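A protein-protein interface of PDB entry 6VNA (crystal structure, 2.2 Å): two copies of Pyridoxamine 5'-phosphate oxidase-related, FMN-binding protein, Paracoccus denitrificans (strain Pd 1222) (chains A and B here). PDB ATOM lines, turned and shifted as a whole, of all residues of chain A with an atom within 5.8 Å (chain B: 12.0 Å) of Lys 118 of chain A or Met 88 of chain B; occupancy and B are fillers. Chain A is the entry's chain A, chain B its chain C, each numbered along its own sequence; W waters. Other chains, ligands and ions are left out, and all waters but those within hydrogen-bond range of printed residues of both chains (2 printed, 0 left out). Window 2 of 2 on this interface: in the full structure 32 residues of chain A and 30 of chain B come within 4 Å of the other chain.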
ATOM      1  N   HIS A  26     -20.322  -8.428  -2.744  1.00  0.00           N
ATOM      2  CA  HIS A  26     -20.474  -7.092  -2.122  1.00  0.00           C
ATOM      3  C   HIS A  26     -21.271  -7.234  -0.842  1.00  0.00           C
ATOM      4  O   HIS A  26     -21.899  -8.287  -0.676  1.00  0.00           O
ATOM      5  CB  HIS A  26     -21.161  -6.104  -3.073  1.00  0.00           C
ATOM      6  CG  HIS A  26     -20.471  -6.011  -4.384  1.00  0.00           C
ATOM      7  ND1 HIS A  26     -19.280  -5.336  -4.533  1.00  0.00           N
ATOM      8  CD2 HIS A  26     -20.783  -6.525  -5.601  1.00  0.00           C
ATOM      9  CE1 HIS A  26     -18.876  -5.436  -5.787  1.00  0.00           C
ATOM     10  NE2 HIS A  26     -19.788  -6.155  -6.466  1.00  0.00           N
ATOM     11  N   ARG A  43     -21.192   0.612   1.363  1.00  0.00           N
ATOM     12  CA  ARG A  43     -21.168  -0.556   0.456  1.00  0.00           C
ATOM     13  C   ARG A  43     -19.713  -0.924   0.194  1.00  0.00           C
ATOM     14  O   ARG A  43     -18.958  -0.021  -0.166  1.00  0.00           O
ATOM     15  CB  ARG A  43     -21.880  -0.260  -0.867  1.00  0.00           C
ATOM     16  CG  ARG A  43     -21.887  -1.461  -1.796  1.00  0.00           C
ATOM     17  CD  ARG A  43     -22.707  -1.192  -3.022  1.00  0.00           C
ATOM     18  NE  ARG A  43     -24.121  -1.405  -2.792  1.00  0.00           N
ATOM     19  CZ  ARG A  43     -25.081  -1.061  -3.646  1.00  0.00           C
ATOM     20  NH1 ARG A  43     -24.776  -0.473  -4.791  1.00  0.00           N
ATOM     21  NH2 ARG A  43     -26.348  -1.317  -3.355  1.00  0.00           N
ATOM     22  N   ILE A  44     -19.376  -2.202   0.321  1.00  0.00           N
ATOM     23  CA  ILE A  44     -17.985  -2.713   0.156  1.00  0.00           C
ATOM     24  C   ILE A  44     -17.933  -3.962  -0.734  1.00  0.00           C
ATOM     25  O   ILE A  44     -18.904  -4.728  -0.780  1.00  0.00           O
ATOM     26  CB  ILE A  44     -17.373  -3.038   1.529  1.00  0.00           C
ATOM     27  CG1 ILE A  44     -18.169  -4.118   2.268  1.00  0.00           C
ATOM     28  CG2 ILE A  44     -17.222  -1.773   2.356  1.00  0.00           C
ATOM     29  CD1 ILE A  44     -17.335  -4.957   3.207  1.00  0.00           C
ATOM     30  N   ALA A  45     -16.788  -4.179  -1.360  1.00  0.00           N
ATOM     31  CA  ALA A  45     -16.421  -5.474  -1.971  1.00  0.00           C
ATOM     32  C   ALA A  45     -16.159  -6.435  -0.816  1.00  0.00           C
ATOM     33  O   ALA A  45     -15.454  -6.054   0.130  1.00  0.00           O
ATOM     34  CB  ALA A  45     -15.232  -5.329  -2.888  1.00  0.00           C
ATOM     35  N   LEU A 113      -9.829 -12.110  -7.694  1.00  0.00           N
ATOM     36  CA  LEU A 113     -10.063 -11.684  -9.104  1.00  0.00           C
ATOM     37  C   LEU A 113     -10.845 -12.772  -9.858  1.00  0.00           C
ATOM     38  O   LEU A 113     -11.806 -12.422 -10.587  1.00  0.00           O
ATOM     39  CB  LEU A 113      -8.735 -11.352  -9.787  1.00  0.00           C
ATOM     40  CG  LEU A 113      -8.845 -10.353 -10.941  1.00  0.00           C
ATOM     41  CD1 LEU A 113      -9.313  -8.992 -10.438  1.00  0.00           C
ATOM     42  CD2 LEU A 113      -7.521 -10.220 -11.682  1.00  0.00           C
ATOM     43  N   ASP A 116     -14.186 -11.972  -8.712  1.00  0.00           N
ATOM     44  CA  ASP A 116     -14.634 -10.596  -9.055  1.00  0.00           C
ATOM     45  C   ASP A 116     -13.600  -9.973  -9.991  1.00  0.00           C
ATOM     46  O   ASP A 116     -12.648  -9.344  -9.524  1.00  0.00           O
ATOM     47  CB  ASP A 116     -14.858  -9.775  -7.783  1.00  0.00           C
ATOM     48  CG  ASP A 116     -15.617  -8.478  -7.993  1.00  0.00           C
ATOM     49  OD1 ASP A 116     -16.050  -8.229  -9.136  1.00  0.00           O
ATOM     50  OD2 ASP A 116     -15.776  -7.730  -7.000  1.00  0.00           O
ATOM     51  N   PRO A 117     -13.736 -10.169 -11.329  1.00  0.00           N
ATOM     52  CA  PRO A 117     -12.799  -9.599 -12.303  1.00  0.00           C
ATOM     53  C   PRO A 117     -12.729  -8.060 -12.263  1.00  0.00           C
ATOM     54  O   PRO A 117     -11.630  -7.524 -12.170  1.00  0.00           O
ATOM     55  CB  PRO A 117     -13.352 -10.076 -13.658  1.00  0.00           C
ATOM     56  CG  PRO A 117     -14.215 -11.274 -13.332  1.00  0.00           C
ATOM     57  CD  PRO A 117     -14.785 -10.981 -11.967  1.00  0.00           C
ATOM     58  N   LYS A 118     -13.893  -7.398 -12.320  1.00  0.00           N
ATOM     59  CA  LYS A 118     -14.081  -5.927 -12.153  1.00  0.00           C
ATOM     60  C   LYS A 118     -13.123  -5.368 -11.088  1.00  0.00           C
ATOM     61  O   LYS A 118     -12.662  -4.219 -11.264  1.00  0.00           O
ATOM     62  CB  LYS A 118     -15.540  -5.631 -11.777  1.00  0.00           C
ATOM     63  CG  LYS A 118     -15.859  -4.184 -11.407  1.00  0.00           C
ATOM     64  CD  LYS A 118     -15.685  -3.825  -9.929  1.00  0.00           C
ATOM     65  CE  LYS A 118     -16.759  -4.389  -9.017  1.00  0.00           C
ATOM     66  NZ  LYS A 118     -16.243  -4.622  -7.648  1.00  0.00           N
ATOM     67  N   ALA A 119     -12.844  -6.137 -10.026  1.00  0.00           N
ATOM     68  CA  ALA A 119     -12.043  -5.726  -8.846  1.00  0.00           C
ATOM     69  C   ALA A 119     -10.536  -5.731  -9.152  1.00  0.00           C
ATOM     70  O   ALA A 119      -9.754  -5.874  -8.189  1.00  0.00           O
ATOM     71  CB  ALA A 119     -12.364  -6.626  -7.673  1.00  0.00           C
ATOM     72  N   LYS A 120     -10.129  -5.559 -10.418  1.00  0.00           N
ATOM     73  CA  LYS A 120      -8.721  -5.234 -10.778  1.00  0.00           C
ATOM     74  C   LYS A 120      -8.482  -3.738 -10.534  1.00  0.00           C
ATOM     75  O   LYS A 120      -7.423  -3.389  -9.959  1.00  0.00           O
ATOM     76  CB  LYS A 120      -8.394  -5.592 -12.231  1.00  0.00           C
ATOM     77  CG  LYS A 120      -6.903  -5.698 -12.557  1.00  0.00           C
ATOM     78  CD  LYS A 120      -5.991  -4.817 -11.695  1.00  0.00           C
ATOM     79  CE  LYS A 120      -4.540  -4.763 -12.123  1.00  0.00           C
ATOM     80  NZ  LYS A 120      -4.235  -3.505 -12.846  1.00  0.00           N
ATOM     81  N   VAL A 121      -9.426  -2.886 -10.942  1.00  0.00           N
ATOM     82  CA  VAL A 121      -9.390  -1.411 -10.682  1.00  0.00           C
ATOM     83  C   VAL A 121      -8.828  -1.169  -9.267  1.00  0.00           C
ATOM     84  O   VAL A 121      -7.850  -0.413  -9.150  1.00  0.00           O
ATOM     85  CB  VAL A 121     -10.769  -0.747 -10.920  1.00  0.00           C
ATOM     86  CG1 VAL A 121     -11.827  -1.194  -9.922  1.00  0.00           C
ATOM     87  CG2 VAL A 121     -10.678   0.773 -10.945  1.00  0.00           C
ATOM     88  N   TYR A 122      -9.356  -1.849  -8.242  1.00  0.00           N
ATOM     89  CA  TYR A 122      -8.965  -1.685  -6.815  1.00  0.00           C
ATOM     90  C   TYR A 122      -7.540  -2.197  -6.553  1.00  0.00           C
ATOM     91  O   TYR A 122      -6.870  -1.603  -5.687  1.00  0.00           O
ATOM     92  CB  TYR A 122      -9.972  -2.388  -5.904  1.00  0.00           C
ATOM     93  CG  TYR A 122     -11.343  -1.761  -5.876  1.00  0.00           C
ATOM     94  CD1 TYR A 122     -11.536  -0.429  -6.215  1.00  0.00           C
ATOM     95  CD2 TYR A 122     -12.448  -2.493  -5.468  1.00  0.00           C
ATOM     96  CE1 TYR A 122     -12.790   0.155  -6.171  1.00  0.00           C
ATOM     97  CE2 TYR A 122     -13.710  -1.923  -5.412  1.00  0.00           C
ATOM     98  CZ  TYR A 122     -13.878  -0.595  -5.765  1.00  0.00           C
ATOM     99  OH  TYR A 122     -15.106  -0.009  -5.711  1.00  0.00           O
ATOM    100  N   LEU B  16     -28.481  15.157  -6.254  1.00  0.00           N
ATOM    101  CA  LEU B  16     -28.239  13.687  -6.323  1.00  0.00           C
ATOM    102  C   LEU B  16     -28.684  12.993  -5.018  1.00  0.00           C
ATOM    103  O   LEU B  16     -29.382  11.952  -5.105  1.00  0.00           O
ATOM    104  CB  LEU B  16     -26.752  13.438  -6.588  1.00  0.00           C
ATOM    105  CG  LEU B  16     -26.369  11.985  -6.845  1.00  0.00           C
ATOM    106  CD1 LEU B  16     -27.334  11.338  -7.815  1.00  0.00           C
ATOM    107  CD2 LEU B  16     -24.950  11.893  -7.376  1.00  0.00           C
ATOM    108  N   LEU B  20     -31.727  10.277  -4.778  1.00  0.00           N
ATOM    109  CA  LEU B  20     -31.590   8.925  -4.161  1.00  0.00           C
ATOM    110  C   LEU B  20     -32.604   8.763  -3.021  1.00  0.00           C
ATOM    111  O   LEU B  20     -33.256   7.704  -2.917  1.00  0.00           O
ATOM    112  CB  LEU B  20     -30.161   8.746  -3.650  1.00  0.00           C
ATOM    113  CG  LEU B  20     -29.125   8.490  -4.737  1.00  0.00           C
ATOM    114  CD1 LEU B  20     -27.714   8.648  -4.196  1.00  0.00           C
ATOM    115  CD2 LEU B  20     -29.320   7.109  -5.329  1.00  0.00           C
ATOM    116  N   LEU B  77     -27.981   3.379   4.564  1.00  0.00           N
ATOM    117  CA  LEU B  77     -27.298   3.369   3.248  1.00  0.00           C
ATOM    118  C   LEU B  77     -28.393   3.252   2.189  1.00  0.00           C
ATOM    119  O   LEU B  77     -29.244   2.343   2.299  1.00  0.00           O
ATOM    120  CB  LEU B  77     -26.311   2.201   3.174  1.00  0.00           C
ATOM    121  CG  LEU B  77     -25.707   1.933   1.798  1.00  0.00           C
ATOM    122  CD1 LEU B  77     -24.873   3.109   1.337  1.00  0.00           C
ATOM    123  CD2 LEU B  77     -24.861   0.665   1.792  1.00  0.00           C
ATOM    124  N   ILE B  78     -28.408   4.191   1.249  1.00  0.00           N
ATOM    125  CA  ILE B  78     -29.396   4.231   0.142  1.00  0.00           C
ATOM    126  C   ILE B  78     -28.604   4.136  -1.159  1.00  0.00           C
ATOM    127  O   ILE B  78     -27.707   4.980  -1.365  1.00  0.00           O
ATOM    128  CB  ILE B  78     -30.281   5.480   0.282  1.00  0.00           C
ATOM    129  CG1 ILE B  78     -30.991   5.474   1.640  1.00  0.00           C
ATOM    130  CG2 ILE B  78     -31.281   5.570  -0.861  1.00  0.00           C
ATOM    131  CD1 ILE B  78     -31.747   6.743   1.949  1.00  0.00           C
ATOM    132  N   ALA B  79     -28.844   3.067  -1.926  1.00  0.00           N
ATOM    133  CA  ALA B  79     -28.247   2.813  -3.258  1.00  0.00           C
ATOM    134  C   ALA B  79     -29.369   2.612  -4.284  1.00  0.00           C
ATOM    135  O   ALA B  79     -29.340   3.379  -5.274  1.00  0.00           O
ATOM    136  CB  ALA B  79     -27.309   1.633  -3.193  1.00  0.00           C
ATOM    137  N   ALA B  87     -21.516  -3.276  -8.378  1.00  0.00           N
ATOM    138  CA  ALA B  87     -22.307  -2.610  -7.314  1.00  0.00           C
ATOM    139  C   ALA B  87     -21.585  -1.354  -6.807  1.00  0.00           C
ATOM    140  O   ALA B  87     -22.238  -0.544  -6.113  1.00  0.00           O
ATOM    141  CB  ALA B  87     -22.575  -3.576  -6.181  1.00  0.00           C
ATOM    142  N   MET B  88     -20.305  -1.181  -7.153  1.00  0.00           N
ATOM    143  CA  MET B  88     -19.412  -0.143  -6.562  1.00  0.00           C
ATOM    144  C   MET B  88     -19.466   1.165  -7.367  1.00  0.00           C
ATOM    145  O   MET B  88     -18.962   2.185  -6.846  1.00  0.00           O
ATOM    146  CB  MET B  88     -17.960  -0.633  -6.520  1.00  0.00           C
ATOM    147  CG  MET B  88     -17.752  -1.946  -5.764  1.00  0.00           C
ATOM    148  SD  MET B  88     -18.453  -1.957  -4.093  1.00  0.00           S
ATOM    149  CE  MET B  88     -17.678  -0.494  -3.412  1.00  0.00           C
ATOM    150  N   THR B  89     -20.014   1.144  -8.589  1.00  0.00           N
ATOM    151  CA  THR B  89     -20.122   2.337  -9.477  1.00  0.00           C
ATOM    152  C   THR B  89     -21.467   3.044  -9.253  1.00  0.00           C
ATOM    153  O   THR B  89     -21.603   4.172  -9.729  1.00  0.00           O
ATOM    154  CB  THR B  89     -19.908   1.939 -10.942  1.00  0.00           C
ATOM    155  OG1 THR B  89     -20.950   1.017 -11.270  1.00  0.00           O
ATOM    156  CG2 THR B  89     -18.547   1.325 -11.190  1.00  0.00           C
ATOM    157  N   HIS B  90     -22.406   2.391  -8.562  1.00  0.00           N
ATOM    158  CA  HIS B  90     -23.722   2.930  -8.127  1.00  0.00           C
ATOM    159  C   HIS B  90     -23.504   4.150  -7.218  1.00  0.00           C
ATOM    160  O   HIS B  90     -22.739   4.033  -6.263  1.00  0.00           O
ATOM    161  CB  HIS B  90     -24.534   1.858  -7.371  1.00  0.00           C
ATOM    162  CG  HIS B  90     -24.951   0.662  -8.171  1.00  0.00           C
ATOM    163  ND1 HIS B  90     -25.838  -0.290  -7.671  1.00  0.00           N
ATOM    164  CD2 HIS B  90     -24.631   0.253  -9.422  1.00  0.00           C
ATOM    165  CE1 HIS B  90     -26.030  -1.231  -8.574  1.00  0.00           C
ATOM    166  NE2 HIS B  90     -25.301  -0.921  -9.659  1.00  0.00           N
ATOM    167  N   ALA B  91     -24.168   5.275  -7.495  1.00  0.00           N
ATOM    168  CA  ALA B  91     -24.275   6.429  -6.579  1.00  0.00           C
ATOM    169  C   ALA B  91     -24.967   5.965  -5.295  1.00  0.00           C
ATOM    170  O   ALA B  91     -25.949   5.206  -5.369  1.00  0.00           O
ATOM    171  CB  ALA B  91     -25.032   7.557  -7.225  1.00  0.00           C
ATOM    172  N   ARG B  92     -24.473   6.406  -4.144  1.00  0.00           N
ATOM    173  CA  ARG B  92     -25.066   5.998  -2.853  1.00  0.00           C
ATOM    174  C   ARG B  92     -24.820   7.054  -1.791  1.00  0.00           C
ATOM    175  O   ARG B  92     -23.939   7.895  -1.940  1.00  0.00           O
ATOM    176  CB  ARG B  92     -24.483   4.663  -2.391  1.00  0.00           C
ATOM    177  CG  ARG B  92     -22.999   4.513  -2.673  1.00  0.00           C
ATOM    178  CD  ARG B  92     -22.639   3.049  -2.644  1.00  0.00           C
ATOM    179  NE  ARG B  92     -21.197   2.989  -2.592  1.00  0.00           N
ATOM    180  CZ  ARG B  92     -20.383   2.988  -3.644  1.00  0.00           C
ATOM    181  NH1 ARG B  92     -20.849   2.994  -4.880  1.00  0.00           N
ATOM    182  NH2 ARG B  92     -19.081   2.934  -3.450  1.00  0.00           N
ATOM    183  N   LEU B  93     -25.568   6.923  -0.713  1.00  0.00           N
ATOM    184  CA  LEU B  93     -25.686   7.958   0.310  1.00  0.00           C
ATOM    185  C   LEU B  93     -25.748   7.258   1.657  1.00  0.00           C
ATOM    186  O   LEU B  93     -26.632   6.431   1.848  1.00  0.00           O
ATOM    187  CB  LEU B  93     -26.954   8.740  -0.023  1.00  0.00           C
ATOM    188  CG  LEU B  93     -27.388   9.788   0.992  1.00  0.00           C
ATOM    189  CD1 LEU B  93     -26.305  10.838   1.189  1.00  0.00           C
ATOM    190  CD2 LEU B  93     -28.675  10.429   0.518  1.00  0.00           C
ATOM    191  N   SER B  94     -24.785   7.564   2.522  1.00  0.00           N
ATOM    192  CA  SER B  94     -24.747   7.170   3.946  1.00  0.00           C
ATOM    193  C   SER B  94     -25.292   8.332   4.790  1.00  0.00           C
ATOM    194  O   SER B  94     -24.893   9.460   4.556  1.00  0.00           O
ATOM    195  CB  SER B  94     -23.351   6.809   4.340  1.00  0.00           C
ATOM    196  OG  SER B  94     -22.879   5.727   3.560  1.00  0.00           O
ATOM    197  N   LEU B 139     -22.727  11.264   3.842  1.00  0.00           N
ATOM    198  CA  LEU B 139     -21.566  10.964   2.968  1.00  0.00           C
ATOM    199  C   LEU B 139     -22.132  10.520   1.619  1.00  0.00           C
ATOM    200  O   LEU B 139     -22.885   9.541   1.602  1.00  0.00           O
ATOM    201  CB  LEU B 139     -20.752   9.857   3.644  1.00  0.00           C
ATOM    202  CG  LEU B 139     -19.276  10.158   3.864  1.00  0.00           C
ATOM    203  CD1 LEU B 139     -19.105  11.379   4.752  1.00  0.00           C
ATOM    204  CD2 LEU B 139     -18.572   8.952   4.467  1.00  0.00           C
ATOM    205  N   LEU B 140     -21.906  11.293   0.562  1.00  0.00           N
ATOM    206  CA  LEU B 140     -22.422  10.975  -0.793  1.00  0.00           C
ATOM    207  C   LEU B 140     -21.261  10.444  -1.630  1.00  0.00           C
ATOM    208  O   LEU B 140     -20.240  11.160  -1.762  1.00  0.00           O
ATOM    209  CB  LEU B 140     -23.029  12.212  -1.456  1.00  0.00           C
ATOM    210  CG  LEU B 140     -23.437  12.010  -2.917  1.00  0.00           C
ATOM    211  CD1 LEU B 140     -24.726  11.214  -3.004  1.00  0.00           C
ATOM    212  CD2 LEU B 140     -23.580  13.333  -3.637  1.00  0.00           C
ATOM    213  N   ASN B 141     -21.429   9.247  -2.181  1.00  0.00           N
ATOM    214  CA  ASN B 141     -20.461   8.636  -3.122  1.00  0.00           C
ATOM    215  C   ASN B 141     -21.149   8.598  -4.487  1.00  0.00           C
ATOM    216  O   ASN B 141     -22.156   7.865  -4.605  1.00  0.00           O
ATOM    217  CB  ASN B 141     -20.005   7.268  -2.609  1.00  0.00           C
ATOM    218  CG  ASN B 141     -18.911   6.649  -3.451  1.00  0.00           C
ATOM    219  OD1 ASN B 141     -18.830   6.878  -4.653  1.00  0.00           O
ATOM    220  ND2 ASN B 141     -18.059   5.856  -2.829  1.00  0.00           N
ATOM    221  N   ALA B 142     -20.664   9.390  -5.448  1.00  0.00           N
ATOM    222  CA  ALA B 142     -21.053   9.324  -6.877  1.00  0.00           C
ATOM    223  C   ALA B 142     -20.167   8.305  -7.617  1.00  0.00           C
ATOM    224  O   ALA B 142     -20.719   7.262  -8.049  1.00  0.00           O
ATOM    225  CB  ALA B 142     -20.969  10.695  -7.499  1.00  0.00           C
ATOM    226  N   GLY B 143     -18.853   8.583  -7.715  1.00  0.00           N
ATOM    227  CA  GLY B 143     -17.871   7.898  -8.591  1.00  0.00           C
ATOM    228  C   GLY B 143     -17.544   6.492  -8.123  1.00  0.00           C
ATOM    229  O   GLY B 143     -18.263   5.569  -8.566  1.00  0.00           O
ATOM    230  N   ALA B 147     -15.772  11.195  -2.696  1.00  0.00           N
ATOM    231  CA  ALA B 147     -16.975  11.395  -1.856  1.00  0.00           C
ATOM    232  C   ALA B 147     -17.216  12.886  -1.594  1.00  0.00           C
ATOM    233  O   ALA B 147     -16.464  13.730  -2.122  1.00  0.00           O
ATOM    234  CB  ALA B 147     -16.839  10.631  -0.563  1.00  0.00           C
HETATM  235  O   HOH W   1     -20.869   3.471   0.173  1.00  0.00           O
HETATM  236  O   HOH W   2     -18.526   2.692  -0.573  1.00  0.00           O
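A ring nitrogen (ND1) of His 90 of chain B sits at hydrogen-bond distance from the guanidinium group (NH1) of Arg 43 of chain A, 3.1 Å away. ND1 of His 26 of chain A sits at hydrogen-bond distance from SD of Met 88 of chain B (3.5 Å). The guanidinium group of Arg 43 of chain A lies within hydrogen-bond range of the backbone carbonyl oxygen of Ala 87 of chain B, at 2.9 Å.
N of Arg 92 of chain B lies within hydrogen-bond range of O of Asn 141 of chain B (2.8 Å). The backbone carbonyl oxygen (O) of Met 88 of chain B sits at hydrogen-bond distance from the guanidinium group (NH1) of Arg 92 of chain B (2.8 Å). The guanidinium group of Arg 92 of chain B lies within hydrogen-bond range of the backbone carbonyl oxygen of His 90 of chain B, at 2.6 Å. OD2 of Asp 116 of chain A is in salt-bridge range of NZ of Lys 118 of chain A, at 3.2 Å.
Ala 87 of chain B touches His 26 of chain A (CB to CD2, 3.5 Å). Arg 43 of chain A touches Leu 77 of chain B. NH2 of Arg 43 of chain A touches CB of Ala 79 of chain B, at 3.1 Å. Arg 43 of chain A touches Met 88 of chain B (O to CE, 3.5 Å). Arg 43 of chain A touches Arg 92 of chain B (CB to NE, 3.7 Å). SD of Met 88 of chain B touches C of Ile 44 of chain A, 3.9 Å away. N of Ala 45 of chain A touches SD of Met 88 of chain B (3.9 Å). CG of Met 88 of chain B touches NZ of Lys 118 of chain A (3.6 Å). Met 88 of chain B touches Tyr 122 of chain A.
Lys 118 of chain A touches just one residue of chain B: Met 88. Met 88 of chain B touches six residues of chain A. Of the printed residues of chain B, Arg 43 of chain A touches Leu 77, Ala 79, Ala 87, Met 88, His 90 and Arg 92. Of the printed residues of chain B, Ala 45 of chain A touches Met 88 (3.9 Å). No residue of chain B comes within 4 Å of Leu 113 of chain A. Asp 116 of chain A touches none of the printed residues of chain B. No residue of chain B comes within 4 Å of Ala 119 of chain A. No residue of chain B comes within 4 Å of Val 121 of chain A. Printed residues of chain A within 4 Å of Ala 87 of chain B: His 26 and Arg 43. Of the printed residues of chain A, Ala 79 of chain B touches Arg 43. Of the printed residues of chain A, Arg 92 of chain B touches Arg 43. Of the printed residues of chain A, Leu 77 of chain B touches Arg 43. Of the printed residues of chain B, Tyr 122 of chain A touches Met 88 (3.0 Å). Asn 141 of chain B touches none of the printed residues of chain A. The nearest residue of chain B that does not touch Lys 118 of chain A is Ala 87 of chain B (4.9 Å). The nearest printed residue of chain A that does not touch Met 88 of chain B is Asp 116 of chain A (6.2 Å). The nearest printed residue of chain A that does not touch Ala 79 of chain B is Ile 44 of chain A (9.5 Å).
Hydrophobic or aromatic side chains of chain B that line the printed part of chain A: Leu 77, Ala 79, Ala 87, Met 88 and His 90. Along chain B the printed residues that touch a printed residue of chain A span positions 77 to 92. Among the printed residues, 12 pairs touch across the chains. Among the printed residues, no Asp or Glu carboxylate lies within 4 Å of a Lys or Arg side-chain nitrogen of the other chain.
No position is printed for both chains. Of the 12 pairs that touch across the chains among the printed residues, none has its exchanged pair printed and touching as well.
Water W2 lies within hydrogen-bond range of the backbone carbonyl oxygen of Arg 43 of chain A and the guanidinium group of Arg 92 of chain B. Water W1 bridges the guanidinium group of Arg 92 of chain B (2.8 Å) and the backbone NH of Arg 43 of chain A (3.1 Å).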
